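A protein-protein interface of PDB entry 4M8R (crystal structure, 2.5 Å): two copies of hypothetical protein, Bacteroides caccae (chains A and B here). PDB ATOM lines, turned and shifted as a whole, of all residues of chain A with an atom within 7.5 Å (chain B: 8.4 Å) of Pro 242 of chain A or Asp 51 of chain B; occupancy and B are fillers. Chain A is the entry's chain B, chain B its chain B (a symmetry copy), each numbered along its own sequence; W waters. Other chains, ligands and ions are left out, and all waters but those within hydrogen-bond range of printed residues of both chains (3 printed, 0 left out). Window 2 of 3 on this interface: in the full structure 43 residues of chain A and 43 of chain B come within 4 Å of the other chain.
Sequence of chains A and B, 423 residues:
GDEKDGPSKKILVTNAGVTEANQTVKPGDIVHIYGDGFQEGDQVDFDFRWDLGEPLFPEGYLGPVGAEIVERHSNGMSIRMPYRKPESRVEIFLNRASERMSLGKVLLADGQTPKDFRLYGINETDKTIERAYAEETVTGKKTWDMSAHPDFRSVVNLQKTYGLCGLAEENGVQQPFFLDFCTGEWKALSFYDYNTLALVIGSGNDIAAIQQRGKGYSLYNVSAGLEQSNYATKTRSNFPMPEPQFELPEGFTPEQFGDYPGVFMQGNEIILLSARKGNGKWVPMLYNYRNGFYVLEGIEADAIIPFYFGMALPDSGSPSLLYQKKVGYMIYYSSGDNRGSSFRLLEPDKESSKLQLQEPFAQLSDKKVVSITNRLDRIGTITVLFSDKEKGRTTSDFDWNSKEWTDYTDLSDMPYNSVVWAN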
ATOM      1  N   ARG A 213      31.178  -9.573 -30.772  1.00  0.00           N
ATOM      2  CA  ARG A 213      30.636 -10.540 -31.733  1.00  0.00           C
ATOM      3  C   ARG A 213      31.457 -10.604 -33.022  1.00  0.00           C
ATOM      4  O   ARG A 213      31.479 -11.640 -33.694  1.00  0.00           O
ATOM      5  CB  ARG A 213      29.180 -10.194 -32.059  1.00  0.00           C
ATOM      6  CG  ARG A 213      28.439 -11.227 -32.893  1.00  0.00           C
ATOM      7  CD  ARG A 213      26.961 -10.887 -32.989  1.00  0.00           C
ATOM      8  NE  ARG A 213      26.217 -11.927 -33.697  1.00  0.00           N
ATOM      9  CZ  ARG A 213      24.934 -11.844 -34.050  1.00  0.00           C
ATOM     10  NH1 ARG A 213      24.223 -10.762 -33.768  1.00  0.00           N
ATOM     11  NH2 ARG A 213      24.358 -12.853 -34.694  1.00  0.00           N
ATOM     12  N   SER A 218      28.161  -6.568 -29.223  1.00  0.00           N
ATOM     13  CA  SER A 218      26.733  -6.864 -29.189  1.00  0.00           C
ATOM     14  C   SER A 218      26.315  -7.243 -27.778  1.00  0.00           C
ATOM     15  O   SER A 218      27.147  -7.581 -26.938  1.00  0.00           O
ATOM     16  CB  SER A 218      26.400  -8.022 -30.132  1.00  0.00           C
ATOM     17  OG  SER A 218      26.565  -7.645 -31.484  1.00  0.00           O
ATOM     18  N   LEU A 219      25.011  -7.216 -27.539  1.00  0.00           N
ATOM     19  CA  LEU A 219      24.455  -7.586 -26.243  1.00  0.00           C
ATOM     20  C   LEU A 219      24.024  -9.045 -26.266  1.00  0.00           C
ATOM     21  O   LEU A 219      23.316  -9.463 -27.182  1.00  0.00           O
ATOM     22  CB  LEU A 219      23.267  -6.689 -25.924  1.00  0.00           C
ATOM     23  CG  LEU A 219      22.638  -6.853 -24.544  1.00  0.00           C
ATOM     24  CD1 LEU A 219      23.637  -6.501 -23.453  1.00  0.00           C
ATOM     25  CD2 LEU A 219      21.403  -5.978 -24.451  1.00  0.00           C
ATOM     26  N   PHE A 239      23.625 -16.297 -27.454  1.00  0.00           N
ATOM     27  CA  PHE A 239      22.366 -15.606 -27.708  1.00  0.00           C
ATOM     28  C   PHE A 239      22.540 -14.095 -27.833  1.00  0.00           C
ATOM     29  O   PHE A 239      22.148 -13.346 -26.943  1.00  0.00           O
ATOM     30  CB  PHE A 239      21.367 -15.906 -26.580  1.00  0.00           C
ATOM     31  CG  PHE A 239      20.806 -17.298 -26.601  1.00  0.00           C
ATOM     32  CD1 PHE A 239      20.211 -17.805 -27.743  1.00  0.00           C
ATOM     33  CD2 PHE A 239      20.820 -18.079 -25.455  1.00  0.00           C
ATOM     34  CE1 PHE A 239      19.670 -19.077 -27.756  1.00  0.00           C
ATOM     35  CE2 PHE A 239      20.286 -19.355 -25.460  1.00  0.00           C
ATOM     36  CZ  PHE A 239      19.708 -19.853 -26.613  1.00  0.00           C
ATOM     37  N   PRO A 240      23.117 -13.637 -28.945  1.00  0.00           N
ATOM     38  CA  PRO A 240      23.179 -12.197 -29.178  1.00  0.00           C
ATOM     39  C   PRO A 240      21.829 -11.642 -29.605  1.00  0.00           C
ATOM     40  O   PRO A 240      20.989 -12.381 -30.098  1.00  0.00           O
ATOM     41  CB  PRO A 240      24.185 -12.066 -30.325  1.00  0.00           C
ATOM     42  CG  PRO A 240      24.104 -13.368 -31.044  1.00  0.00           C
ATOM     43  CD  PRO A 240      23.810 -14.401 -29.995  1.00  0.00           C
ATOM     44  N   MET A 241      21.637 -10.346 -29.417  1.00  0.00           N
ATOM     45  CA  MET A 241      20.446  -9.665 -29.891  1.00  0.00           C
ATOM     46  C   MET A 241      20.552  -9.476 -31.375  1.00  0.00           C
ATOM     47  O   MET A 241      21.655  -9.327 -31.902  1.00  0.00           O
ATOM     48  CB  MET A 241      20.355  -8.288 -29.260  1.00  0.00           C
ATOM     49  CG  MET A 241      20.135  -8.372 -27.753  1.00  0.00           C
ATOM     50  SD  MET A 241      18.203  -8.441 -27.398  1.00  0.00           S
ATOM     51  CE  MET A 241      18.006  -6.492 -27.424  1.00  0.00           C
ATOM     52  N   PRO A 242      19.408  -9.451 -32.081  1.00  0.00           N
ATOM     53  CA  PRO A 242      19.408  -9.153 -33.512  1.00  0.00           C
ATOM     54  C   PRO A 242      19.535  -7.657 -33.749  1.00  0.00           C
ATOM     55  O   PRO A 242      18.629  -7.029 -34.297  1.00  0.00           O
ATOM     56  CB  PRO A 242      18.038  -9.653 -33.961  1.00  0.00           C
ATOM     57  CG  PRO A 242      17.175  -9.387 -32.777  1.00  0.00           C
ATOM     58  CD  PRO A 242      18.041  -9.672 -31.578  1.00  0.00           C
ATOM     59  N   GLU A 243      20.656  -7.094 -33.327  1.00  0.00           N
ATOM     60  CA  GLU A 243      20.924  -5.672 -33.497  1.00  0.00           C
ATOM     61  C   GLU A 243      22.317  -5.512 -34.089  1.00  0.00           C
ATOM     62  O   GLU A 243      23.133  -6.426 -34.009  1.00  0.00           O
ATOM     63  CB  GLU A 243      20.842  -4.959 -32.146  1.00  0.00           C
ATOM     64  CG  GLU A 243      19.511  -5.118 -31.423  1.00  0.00           C
ATOM     65  CD  GLU A 243      18.352  -4.415 -32.116  1.00  0.00           C
ATOM     66  OE1 GLU A 243      18.597  -3.538 -32.963  1.00  0.00           O
ATOM     67  OE2 GLU A 243      17.184  -4.746 -31.817  1.00  0.00           O
ATOM     68  N   PRO A 244      22.608  -4.347 -34.672  1.00  0.00           N
ATOM     69  CA  PRO A 244      23.947  -4.170 -35.228  1.00  0.00           C
ATOM     70  C   PRO A 244      25.037  -4.194 -34.160  1.00  0.00           C
ATOM     71  O   PRO A 244      24.743  -4.091 -32.964  1.00  0.00           O
ATOM     72  CB  PRO A 244      23.884  -2.784 -35.891  1.00  0.00           C
ATOM     73  CG  PRO A 244      22.440  -2.404 -35.926  1.00  0.00           C
ATOM     74  CD  PRO A 244      21.802  -3.120 -34.780  1.00  0.00           C
ATOM     75  N   TYR A 289      21.502  -0.736 -27.203  1.00  0.00           N
ATOM     76  CA  TYR A 289      21.741  -1.854 -28.127  1.00  0.00           C
ATOM     77  C   TYR A 289      21.261  -1.588 -29.552  1.00  0.00           C
ATOM     78  O   TYR A 289      21.644  -2.308 -30.475  1.00  0.00           O
ATOM     79  CB  TYR A 289      21.176  -3.183 -27.598  1.00  0.00           C
ATOM     80  CG  TYR A 289      19.676  -3.245 -27.352  1.00  0.00           C
ATOM     81  CD1 TYR A 289      18.764  -3.179 -28.404  1.00  0.00           C
ATOM     82  CD2 TYR A 289      19.176  -3.426 -26.068  1.00  0.00           C
ATOM     83  CE1 TYR A 289      17.401  -3.255 -28.180  1.00  0.00           C
ATOM     84  CE2 TYR A 289      17.814  -3.517 -25.837  1.00  0.00           C
ATOM     85  CZ  TYR A 289      16.930  -3.427 -26.892  1.00  0.00           C
ATOM     86  OH  TYR A 289      15.575  -3.515 -26.661  1.00  0.00           O
ATOM     87  N   PHE B  48      17.237 -22.130 -29.792  1.00  0.00           N
ATOM     88  CA  PHE B  48      16.281 -21.229 -30.421  1.00  0.00           C
ATOM     89  C   PHE B  48      16.366 -19.844 -29.792  1.00  0.00           C
ATOM     90  O   PHE B  48      16.508 -19.715 -28.576  1.00  0.00           O
ATOM     91  CB  PHE B  48      14.855 -21.759 -30.248  1.00  0.00           C
ATOM     92  CG  PHE B  48      14.609 -23.091 -30.900  1.00  0.00           C
ATOM     93  CD1 PHE B  48      15.026 -24.262 -30.293  1.00  0.00           C
ATOM     94  CD2 PHE B  48      13.937 -23.172 -32.113  1.00  0.00           C
ATOM     95  CE1 PHE B  48      14.794 -25.492 -30.892  1.00  0.00           C
ATOM     96  CE2 PHE B  48      13.715 -24.388 -32.722  1.00  0.00           C
ATOM     97  CZ  PHE B  48      14.145 -25.554 -32.111  1.00  0.00           C
ATOM     98  N   ARG B  49      16.271 -18.814 -30.629  1.00  0.00           N
ATOM     99  CA  ARG B  49      16.156 -17.438 -30.167  1.00  0.00           C
ATOM    100  C   ARG B  49      15.030 -16.771 -30.950  1.00  0.00           C
ATOM    101  O   ARG B  49      15.047 -16.789 -32.178  1.00  0.00           O
ATOM    102  CB  ARG B  49      17.460 -16.690 -30.400  1.00  0.00           C
ATOM    103  CG  ARG B  49      17.473 -15.284 -29.831  1.00  0.00           C
ATOM    104  CD  ARG B  49      18.454 -14.387 -30.582  1.00  0.00           C
ATOM    105  NE  ARG B  49      18.008 -14.130 -31.954  1.00  0.00           N
ATOM    106  CZ  ARG B  49      18.712 -13.474 -32.873  1.00  0.00           C
ATOM    107  NH1 ARG B  49      19.913 -12.989 -32.587  1.00  0.00           N
ATOM    108  NH2 ARG B  49      18.212 -13.310 -34.091  1.00  0.00           N
ATOM    109  N   TRP B  50      14.060 -16.183 -30.249  1.00  0.00           N
ATOM    110  CA  TRP B  50      12.943 -15.531 -30.923  1.00  0.00           C
ATOM    111  C   TRP B  50      12.498 -14.214 -30.298  1.00  0.00           C
ATOM    112  O   TRP B  50      12.713 -13.964 -29.115  1.00  0.00           O
ATOM    113  CB  TRP B  50      11.754 -16.486 -31.025  1.00  0.00           C
ATOM    114  CG  TRP B  50      11.108 -16.837 -29.721  1.00  0.00           C
ATOM    115  CD1 TRP B  50      10.206 -16.093 -29.039  1.00  0.00           C
ATOM    116  CD2 TRP B  50      11.290 -18.039 -28.968  1.00  0.00           C
ATOM    117  NE1 TRP B  50       9.821 -16.742 -27.892  1.00  0.00           N
ATOM    118  CE2 TRP B  50      10.469 -17.942 -27.825  1.00  0.00           C
ATOM    119  CE3 TRP B  50      12.071 -19.180 -29.143  1.00  0.00           C
ATOM    120  CZ2 TRP B  50      10.402 -18.946 -26.857  1.00  0.00           C
ATOM    121  CZ3 TRP B  50      12.003 -20.189 -28.179  1.00  0.00           C
ATOM    122  CH2 TRP B  50      11.172 -20.060 -27.047  1.00  0.00           C
ATOM    123  N   ASP B  51      11.875 -13.381 -31.130  1.00  0.00           N
ATOM    124  CA  ASP B  51      11.249 -12.137 -30.709  1.00  0.00           C
ATOM    125  C   ASP B  51       9.807 -12.158 -31.194  1.00  0.00           C
ATOM    126  O   ASP B  51       9.571 -12.075 -32.391  1.00  0.00           O
ATOM    127  CB  ASP B  51      11.986 -10.958 -31.336  1.00  0.00           C
ATOM    128  CG  ASP B  51      13.468 -10.974 -31.035  1.00  0.00           C
ATOM    129  OD1 ASP B  51      13.829 -10.724 -29.862  1.00  0.00           O
ATOM    130  OD2 ASP B  51      14.267 -11.232 -31.969  1.00  0.00           O
ATOM    131  N   LEU B  52       8.846 -12.269 -30.282  1.00  0.00           N
ATOM    132  CA  LEU B  52       7.425 -12.357 -30.674  1.00  0.00           C
ATOM    133  C   LEU B  52       6.920 -11.073 -31.338  1.00  0.00           C
ATOM    134  O   LEU B  52       6.274 -11.126 -32.387  1.00  0.00           O
ATOM    135  CB  LEU B  52       6.539 -12.701 -29.473  1.00  0.00           C
ATOM    136  CG  LEU B  52       6.732 -14.096 -28.868  1.00  0.00           C
ATOM    137  CD1 LEU B  52       5.719 -14.353 -27.762  1.00  0.00           C
ATOM    138  CD2 LEU B  52       6.626 -15.178 -29.934  1.00  0.00           C
ATOM    139  N   GLY B  53       7.223  -9.928 -30.733  1.00  0.00           N
ATOM    140  CA  GLY B  53       6.838  -8.636 -31.287  1.00  0.00           C
ATOM    141  C   GLY B  53       8.060  -7.919 -31.807  1.00  0.00           C
ATOM    142  O   GLY B  53       8.728  -8.404 -32.708  1.00  0.00           O
ATOM    143  N   GLU B  54       8.346  -6.751 -31.250  1.00  0.00           N
ATOM    144  CA  GLU B  54       9.596  -6.078 -31.527  1.00  0.00           C
ATOM    145  C   GLU B  54      10.673  -6.646 -30.600  1.00  0.00           C
ATOM    146  O   GLU B  54      10.355  -7.145 -29.519  1.00  0.00           O
ATOM    147  CB  GLU B  54       9.441  -4.565 -31.345  1.00  0.00           C
ATOM    148  CG  GLU B  54       8.376  -3.929 -32.236  1.00  0.00           C
ATOM    149  CD  GLU B  54       8.632  -4.111 -33.728  1.00  0.00           C
ATOM    150  OE1 GLU B  54       9.789  -4.375 -34.128  1.00  0.00           O
ATOM    151  OE2 GLU B  54       7.668  -3.984 -34.514  1.00  0.00           O
ATOM    152  N   PRO B  55      11.951  -6.604 -31.026  1.00  0.00           N
ATOM    153  CA  PRO B  55      13.016  -7.112 -30.163  1.00  0.00           C
ATOM    154  C   PRO B  55      13.193  -6.305 -28.877  1.00  0.00           C
ATOM    155  O   PRO B  55      13.236  -5.078 -28.910  1.00  0.00           O
ATOM    156  CB  PRO B  55      14.274  -6.992 -31.034  1.00  0.00           C
ATOM    157  CG  PRO B  55      13.776  -6.912 -32.433  1.00  0.00           C
ATOM    158  CD  PRO B  55      12.472  -6.186 -32.341  1.00  0.00           C
ATOM    159  N   LEU B  56      13.273  -7.016 -27.757  1.00  0.00           N
ATOM    160  CA  LEU B  56      13.607  -6.437 -26.467  1.00  0.00           C
ATOM    161  C   LEU B  56      14.458  -7.453 -25.703  1.00  0.00           C
ATOM    162  O   LEU B  56      14.379  -8.652 -25.970  1.00  0.00           O
ATOM    163  CB  LEU B  56      12.338  -6.079 -25.686  1.00  0.00           C
ATOM    164  CG  LEU B  56      11.615  -7.181 -24.891  1.00  0.00           C
ATOM    165  CD1 LEU B  56      10.517  -6.573 -24.026  1.00  0.00           C
ATOM    166  CD2 LEU B  56      11.036  -8.272 -25.787  1.00  0.00           C
ATOM    167  N   PHE B  57      15.289  -6.972 -24.782  1.00  0.00           N
ATOM    168  CA  PHE B  57      15.997  -7.854 -23.870  1.00  0.00           C
ATOM    169  C   PHE B  57      15.172  -8.002 -22.594  1.00  0.00           C
ATOM    170  O   PHE B  57      14.746  -7.004 -22.021  1.00  0.00           O
ATOM    171  CB  PHE B  57      17.399  -7.336 -23.528  1.00  0.00           C
ATOM    172  CG  PHE B  57      18.219  -8.335 -22.761  1.00  0.00           C
ATOM    173  CD1 PHE B  57      18.073  -8.467 -21.385  1.00  0.00           C
ATOM    174  CD2 PHE B  57      19.079  -9.199 -23.419  1.00  0.00           C
ATOM    175  CE1 PHE B  57      18.789  -9.418 -20.681  1.00  0.00           C
ATOM    176  CE2 PHE B  57      19.802 -10.151 -22.719  1.00  0.00           C
ATOM    177  CZ  PHE B  57      19.656 -10.259 -21.349  1.00  0.00           C
ATOM    178  N   PRO B  58      14.946  -9.242 -22.135  1.00  0.00           N
ATOM    179  CA  PRO B  58      15.355 -10.513 -22.718  1.00  0.00           C
ATOM    180  C   PRO B  58      14.459 -10.961 -23.862  1.00  0.00           C
ATOM    181  O   PRO B  58      13.265 -10.663 -23.880  1.00  0.00           O
ATOM    182  CB  PRO B  58      15.188 -11.501 -21.555  1.00  0.00           C
ATOM    183  CG  PRO B  58      14.086 -10.928 -20.736  1.00  0.00           C
ATOM    184  CD  PRO B  58      14.247  -9.431 -20.847  1.00  0.00           C
ATOM    185  N   GLU B  59      15.042 -11.701 -24.795  1.00  0.00           N
ATOM    186  CA  GLU B  59      14.293 -12.323 -25.872  1.00  0.00           C
ATOM    187  C   GLU B  59      13.705 -13.634 -25.368  1.00  0.00           C
ATOM    188  O   GLU B  59      13.704 -13.899 -24.175  1.00  0.00           O
ATOM    189  CB  GLU B  59      15.205 -12.572 -27.070  1.00  0.00           C
ATOM    190  CG  GLU B  59      16.007 -11.361 -27.504  1.00  0.00           C
ATOM    191  CD  GLU B  59      16.865 -11.655 -28.713  1.00  0.00           C
ATOM    192  OE1 GLU B  59      16.317 -11.722 -29.830  1.00  0.00           O
ATOM    193  OE2 GLU B  59      18.086 -11.827 -28.539  1.00  0.00           O
ATOM    194  N   GLY B  60      13.170 -14.434 -26.278  1.00  0.00           N
ATOM    195  CA  GLY B  60      12.740 -15.788 -25.959  1.00  0.00           C
ATOM    196  C   GLY B  60      13.850 -16.757 -26.321  1.00  0.00           C
ATOM    197  O   GLY B  60      14.457 -16.632 -27.392  1.00  0.00           O
ATOM    198  N   TYR B  61      14.125 -17.706 -25.425  1.00  0.00           N
ATOM    199  CA  TYR B  61      15.239 -18.633 -25.603  1.00  0.00           C
ATOM    200  C   TYR B  61      14.801 -20.043 -25.319  1.00  0.00           C
ATOM    201  O   TYR B  61      13.956 -20.274 -24.474  1.00  0.00           O
ATOM    202  CB  TYR B  61      16.399 -18.295 -24.664  1.00  0.00           C
ATOM    203  CG  TYR B  61      16.769 -16.843 -24.658  1.00  0.00           C
ATOM    204  CD1 TYR B  61      17.479 -16.284 -25.719  1.00  0.00           C
ATOM    205  CD2 TYR B  61      16.421 -16.026 -23.594  1.00  0.00           C
ATOM    206  CE1 TYR B  61      17.823 -14.944 -25.718  1.00  0.00           C
ATOM    207  CE2 TYR B  61      16.760 -14.686 -23.588  1.00  0.00           C
ATOM    208  CZ  TYR B  61      17.460 -14.152 -24.652  1.00  0.00           C
ATOM    209  OH  TYR B  61      17.791 -12.819 -24.652  1.00  0.00           O
ATOM    210  N   PRO B  86       7.974 -20.586 -32.060  1.00  0.00           N
ATOM    211  CA  PRO B  86       7.781 -19.400 -32.901  1.00  0.00           C
ATOM    212  C   PRO B  86       8.888 -19.261 -33.934  1.00  0.00           C
ATOM    213  O   PRO B  86       9.851 -20.030 -33.910  1.00  0.00           O
ATOM    214  CB  PRO B  86       7.835 -18.239 -31.908  1.00  0.00           C
ATOM    215  CG  PRO B  86       8.495 -18.787 -30.698  1.00  0.00           C
ATOM    216  CD  PRO B  86       8.180 -20.241 -30.645  1.00  0.00           C
ATOM    217  N   GLU B  87       8.736 -18.298 -34.841  1.00  0.00           N
ATOM    218  CA  GLU B  87       9.783 -18.003 -35.804  1.00  0.00           C
ATOM    219  C   GLU B  87      11.066 -17.724 -35.042  1.00  0.00           C
ATOM    220  O   GLU B  87      11.106 -16.838 -34.192  1.00  0.00           O
ATOM    221  CB  GLU B  87       9.422 -16.807 -36.676  1.00  0.00           C
ATOM    222  CG  GLU B  87      10.558 -16.362 -37.589  1.00  0.00           C
ATOM    223  CD  GLU B  87      10.149 -15.277 -38.560  1.00  0.00           C
ATOM    224  OE1 GLU B  87       9.134 -15.462 -39.258  1.00  0.00           O
ATOM    225  OE2 GLU B  87      10.841 -14.244 -38.633  1.00  0.00           O
ATOM    226  N   SER B  88      12.113 -18.478 -35.354  1.00  0.00           N
ATOM    227  CA  SER B  88      13.321 -18.476 -34.540  1.00  0.00           C
ATOM    228  C   SER B  88      14.596 -18.507 -35.351  1.00  0.00           C
ATOM    229  O   SER B  88      14.658 -19.145 -36.401  1.00  0.00           O
ATOM    230  CB  SER B  88      13.327 -19.708 -33.635  1.00  0.00           C
ATOM    231  OG  SER B  88      12.293 -19.645 -32.685  1.00  0.00           O
ATOM    232  N   ARG B  89      15.611 -17.823 -34.834  1.00  0.00           N
ATOM    233  CA  ARG B  89      16.989 -18.091 -35.199  1.00  0.00           C
ATOM    234  C   ARG B  89      17.362 -19.395 -34.510  1.00  0.00           C
ATOM    235  O   ARG B  89      17.354 -19.475 -33.282  1.00  0.00           O
ATOM    236  CB  ARG B  89      17.905 -16.962 -34.725  1.00  0.00           C
ATOM    237  CG  ARG B  89      19.392 -17.299 -34.664  1.00  0.00           C
ATOM    238  CD  ARG B  89      20.173 -16.124 -34.088  1.00  0.00           C
ATOM    239  NE  ARG B  89      21.621 -16.337 -34.031  1.00  0.00           N
ATOM    240  CZ  ARG B  89      22.282 -16.850 -32.995  1.00  0.00           C
ATOM    241  NH1 ARG B  89      21.647 -17.239 -31.888  1.00  0.00           N
ATOM    242  NH2 ARG B  89      23.599 -16.975 -33.068  1.00  0.00           N
ATOM    243  N   ASP B 110       7.569 -19.839 -38.362  1.00  0.00           N
ATOM    244  CA  ASP B 110       6.694 -20.113 -37.225  1.00  0.00           C
ATOM    245  C   ASP B 110       6.085 -21.505 -37.324  1.00  0.00           C
ATOM    246  O   ASP B 110       5.578 -21.888 -38.370  1.00  0.00           O
ATOM    247  CB  ASP B 110       5.581 -19.058 -37.128  1.00  0.00           C
ATOM    248  CG  ASP B 110       4.708 -19.245 -35.898  1.00  0.00           C
ATOM    249  OD1 ASP B 110       3.790 -20.084 -35.934  1.00  0.00           O
ATOM    250  OD2 ASP B 110       4.929 -18.557 -34.889  1.00  0.00           O
HETATM  251  O   HOH W   1      19.652 -11.854 -26.232  1.00  0.00           O
HETATM  252  O   HOH W   2      14.369  -2.973 -31.095  1.00  0.00           O
HETATM  253  O   HOH W   3      14.646  -4.098 -24.122  1.00  0.00           O
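O of Pro 240 of chain A lies within hydrogen-bond range of NH1 of Arg 49 of chain B (2.8 Å). The side-chain carboxylate of Glu 59 of chain B sits close to the backbone carbonyl oxygen of Pro 240 of chain A, 3.3 Å away. The side-chain sulfur (SD) of Met 241 of chain A lies close to the side-chain carboxylate (OE2) of Glu 59 of chain B (3.6 Å).
N of Glu 59 of chain B sits at hydrogen-bond distance from OH of Tyr 61 of chain B (3.0 Å). The backbone carbonyl oxygen of Arg 49 of chain B lies within hydrogen-bond range of the backbone NH of Arg 89 of chain B, at 2.9 Å. The backbone carbonyl oxygen (O) of Met 241 of chain A sits at hydrogen-bond distance from the guanidinium group (NH1) of Arg 213 of chain A, at 3.5 Å. OD1 of Asp 51 of chain B sits close to OE1 of Glu 59 of chain B (2.7 Å). The backbone carbonyl oxygen (O) of Leu 219 of chain A is in hydrogen-bond range of the backbone NH (N) of Met 241 of chain A, at 2.9 Å. NE of Arg 49 of chain B is in salt-bridge range of OE1 of Glu 59 of chain B.
Among the printed residues, pairs that only touch across the chains: Pro 242 of chain A with Glu 59 of chain B (3.2 Å), Phe 239 of chain A with Phe 48 of chain B (3.3 Å), Tyr 289 of chain A with Leu 56 of chain B (3.5 Å), Pro 242 of chain A with Asp 51 of chain B (3.5 Å), Phe 239 of chain A with Tyr 61 of chain B (3.6 Å), Tyr 289 of chain A with Pro 55 of chain B (3.6 Å), Pro 242 of chain A with Arg 49 of chain B (3.6 Å), Glu 243 of chain A with Pro 55 of chain B (3.8 Å), Met 241 of chain A with Arg 49 of chain B (3.8 Å), Met 241 of chain A with Phe 57 of chain B (3.8 Å), Tyr 289 of chain A with Phe 57 of chain B (3.9 Å) and Phe 239 of chain A with Arg 49 of chain B (3.98 Å).
Glu 243 of chain A touches just one residue of chain B: Pro 55. Of chain A, only Pro 242 (3.5 Å) comes within 4 Å of Asp 51 of chain B. Printed residues of chain A within 4 Å of Pro 55 of chain B: Glu 243 (3.8 Å) and Tyr 289 (3.6 Å). Printed residues of chain A within 4 Å of Glu 59 of chain B: Pro 240 (3.3 Å), Met 241 (3.5 Å) and Pro 242 (3.2 Å). Asp 110 of chain B touches none of the printed residues of chain A. The nearest residue of chain B that does not touch Pro 242 of chain A is Pro 55 of chain B (4.1 Å). The nearest residue of chain A that does not touch Asp 51 of chain B is Met 241 of chain A (5.5 Å).
Of the 10 printed residues of chain A, 6 touch a printed residue of chain B. Hydrophobic or aromatic side chains of chain A within 4 Å of the printed part of chain B: Phe 239, Met 241, Pro 242 and Tyr 289. Hydrophobic or aromatic side chains of chain B within 4 Å of the printed part of chain A: Pro 55 and Tyr 61. Among the printed residues, 15 pairs touch across the chains. Among the printed residues, no Asp or Glu carboxylate lies within 4 Å of a Lys or Arg side-chain nitrogen of the other chain.
No position is printed for both chains.
Water W1 lies within hydrogen-bond range of the side-chain hydroxyl (OH) of Tyr 61 of chain B (2.6 Å), the side-chain carboxylate (OE2) of Glu 59 of chain B (2.8 Å) and the backbone carbonyl oxygen (O) of Phe 239 of chain A (3.0 Å). Water W3 lies within hydrogen-bond range of OH of Tyr 289 of chain A (2.8 Å) and N of Phe 57 of chain B (3.0 Å). Water W2 lies within hydrogen-bond range of the backbone carbonyl oxygen (O) of Pro 55 of chain B and the side-chain carboxylate (OE2) of Glu 243 of chain A.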
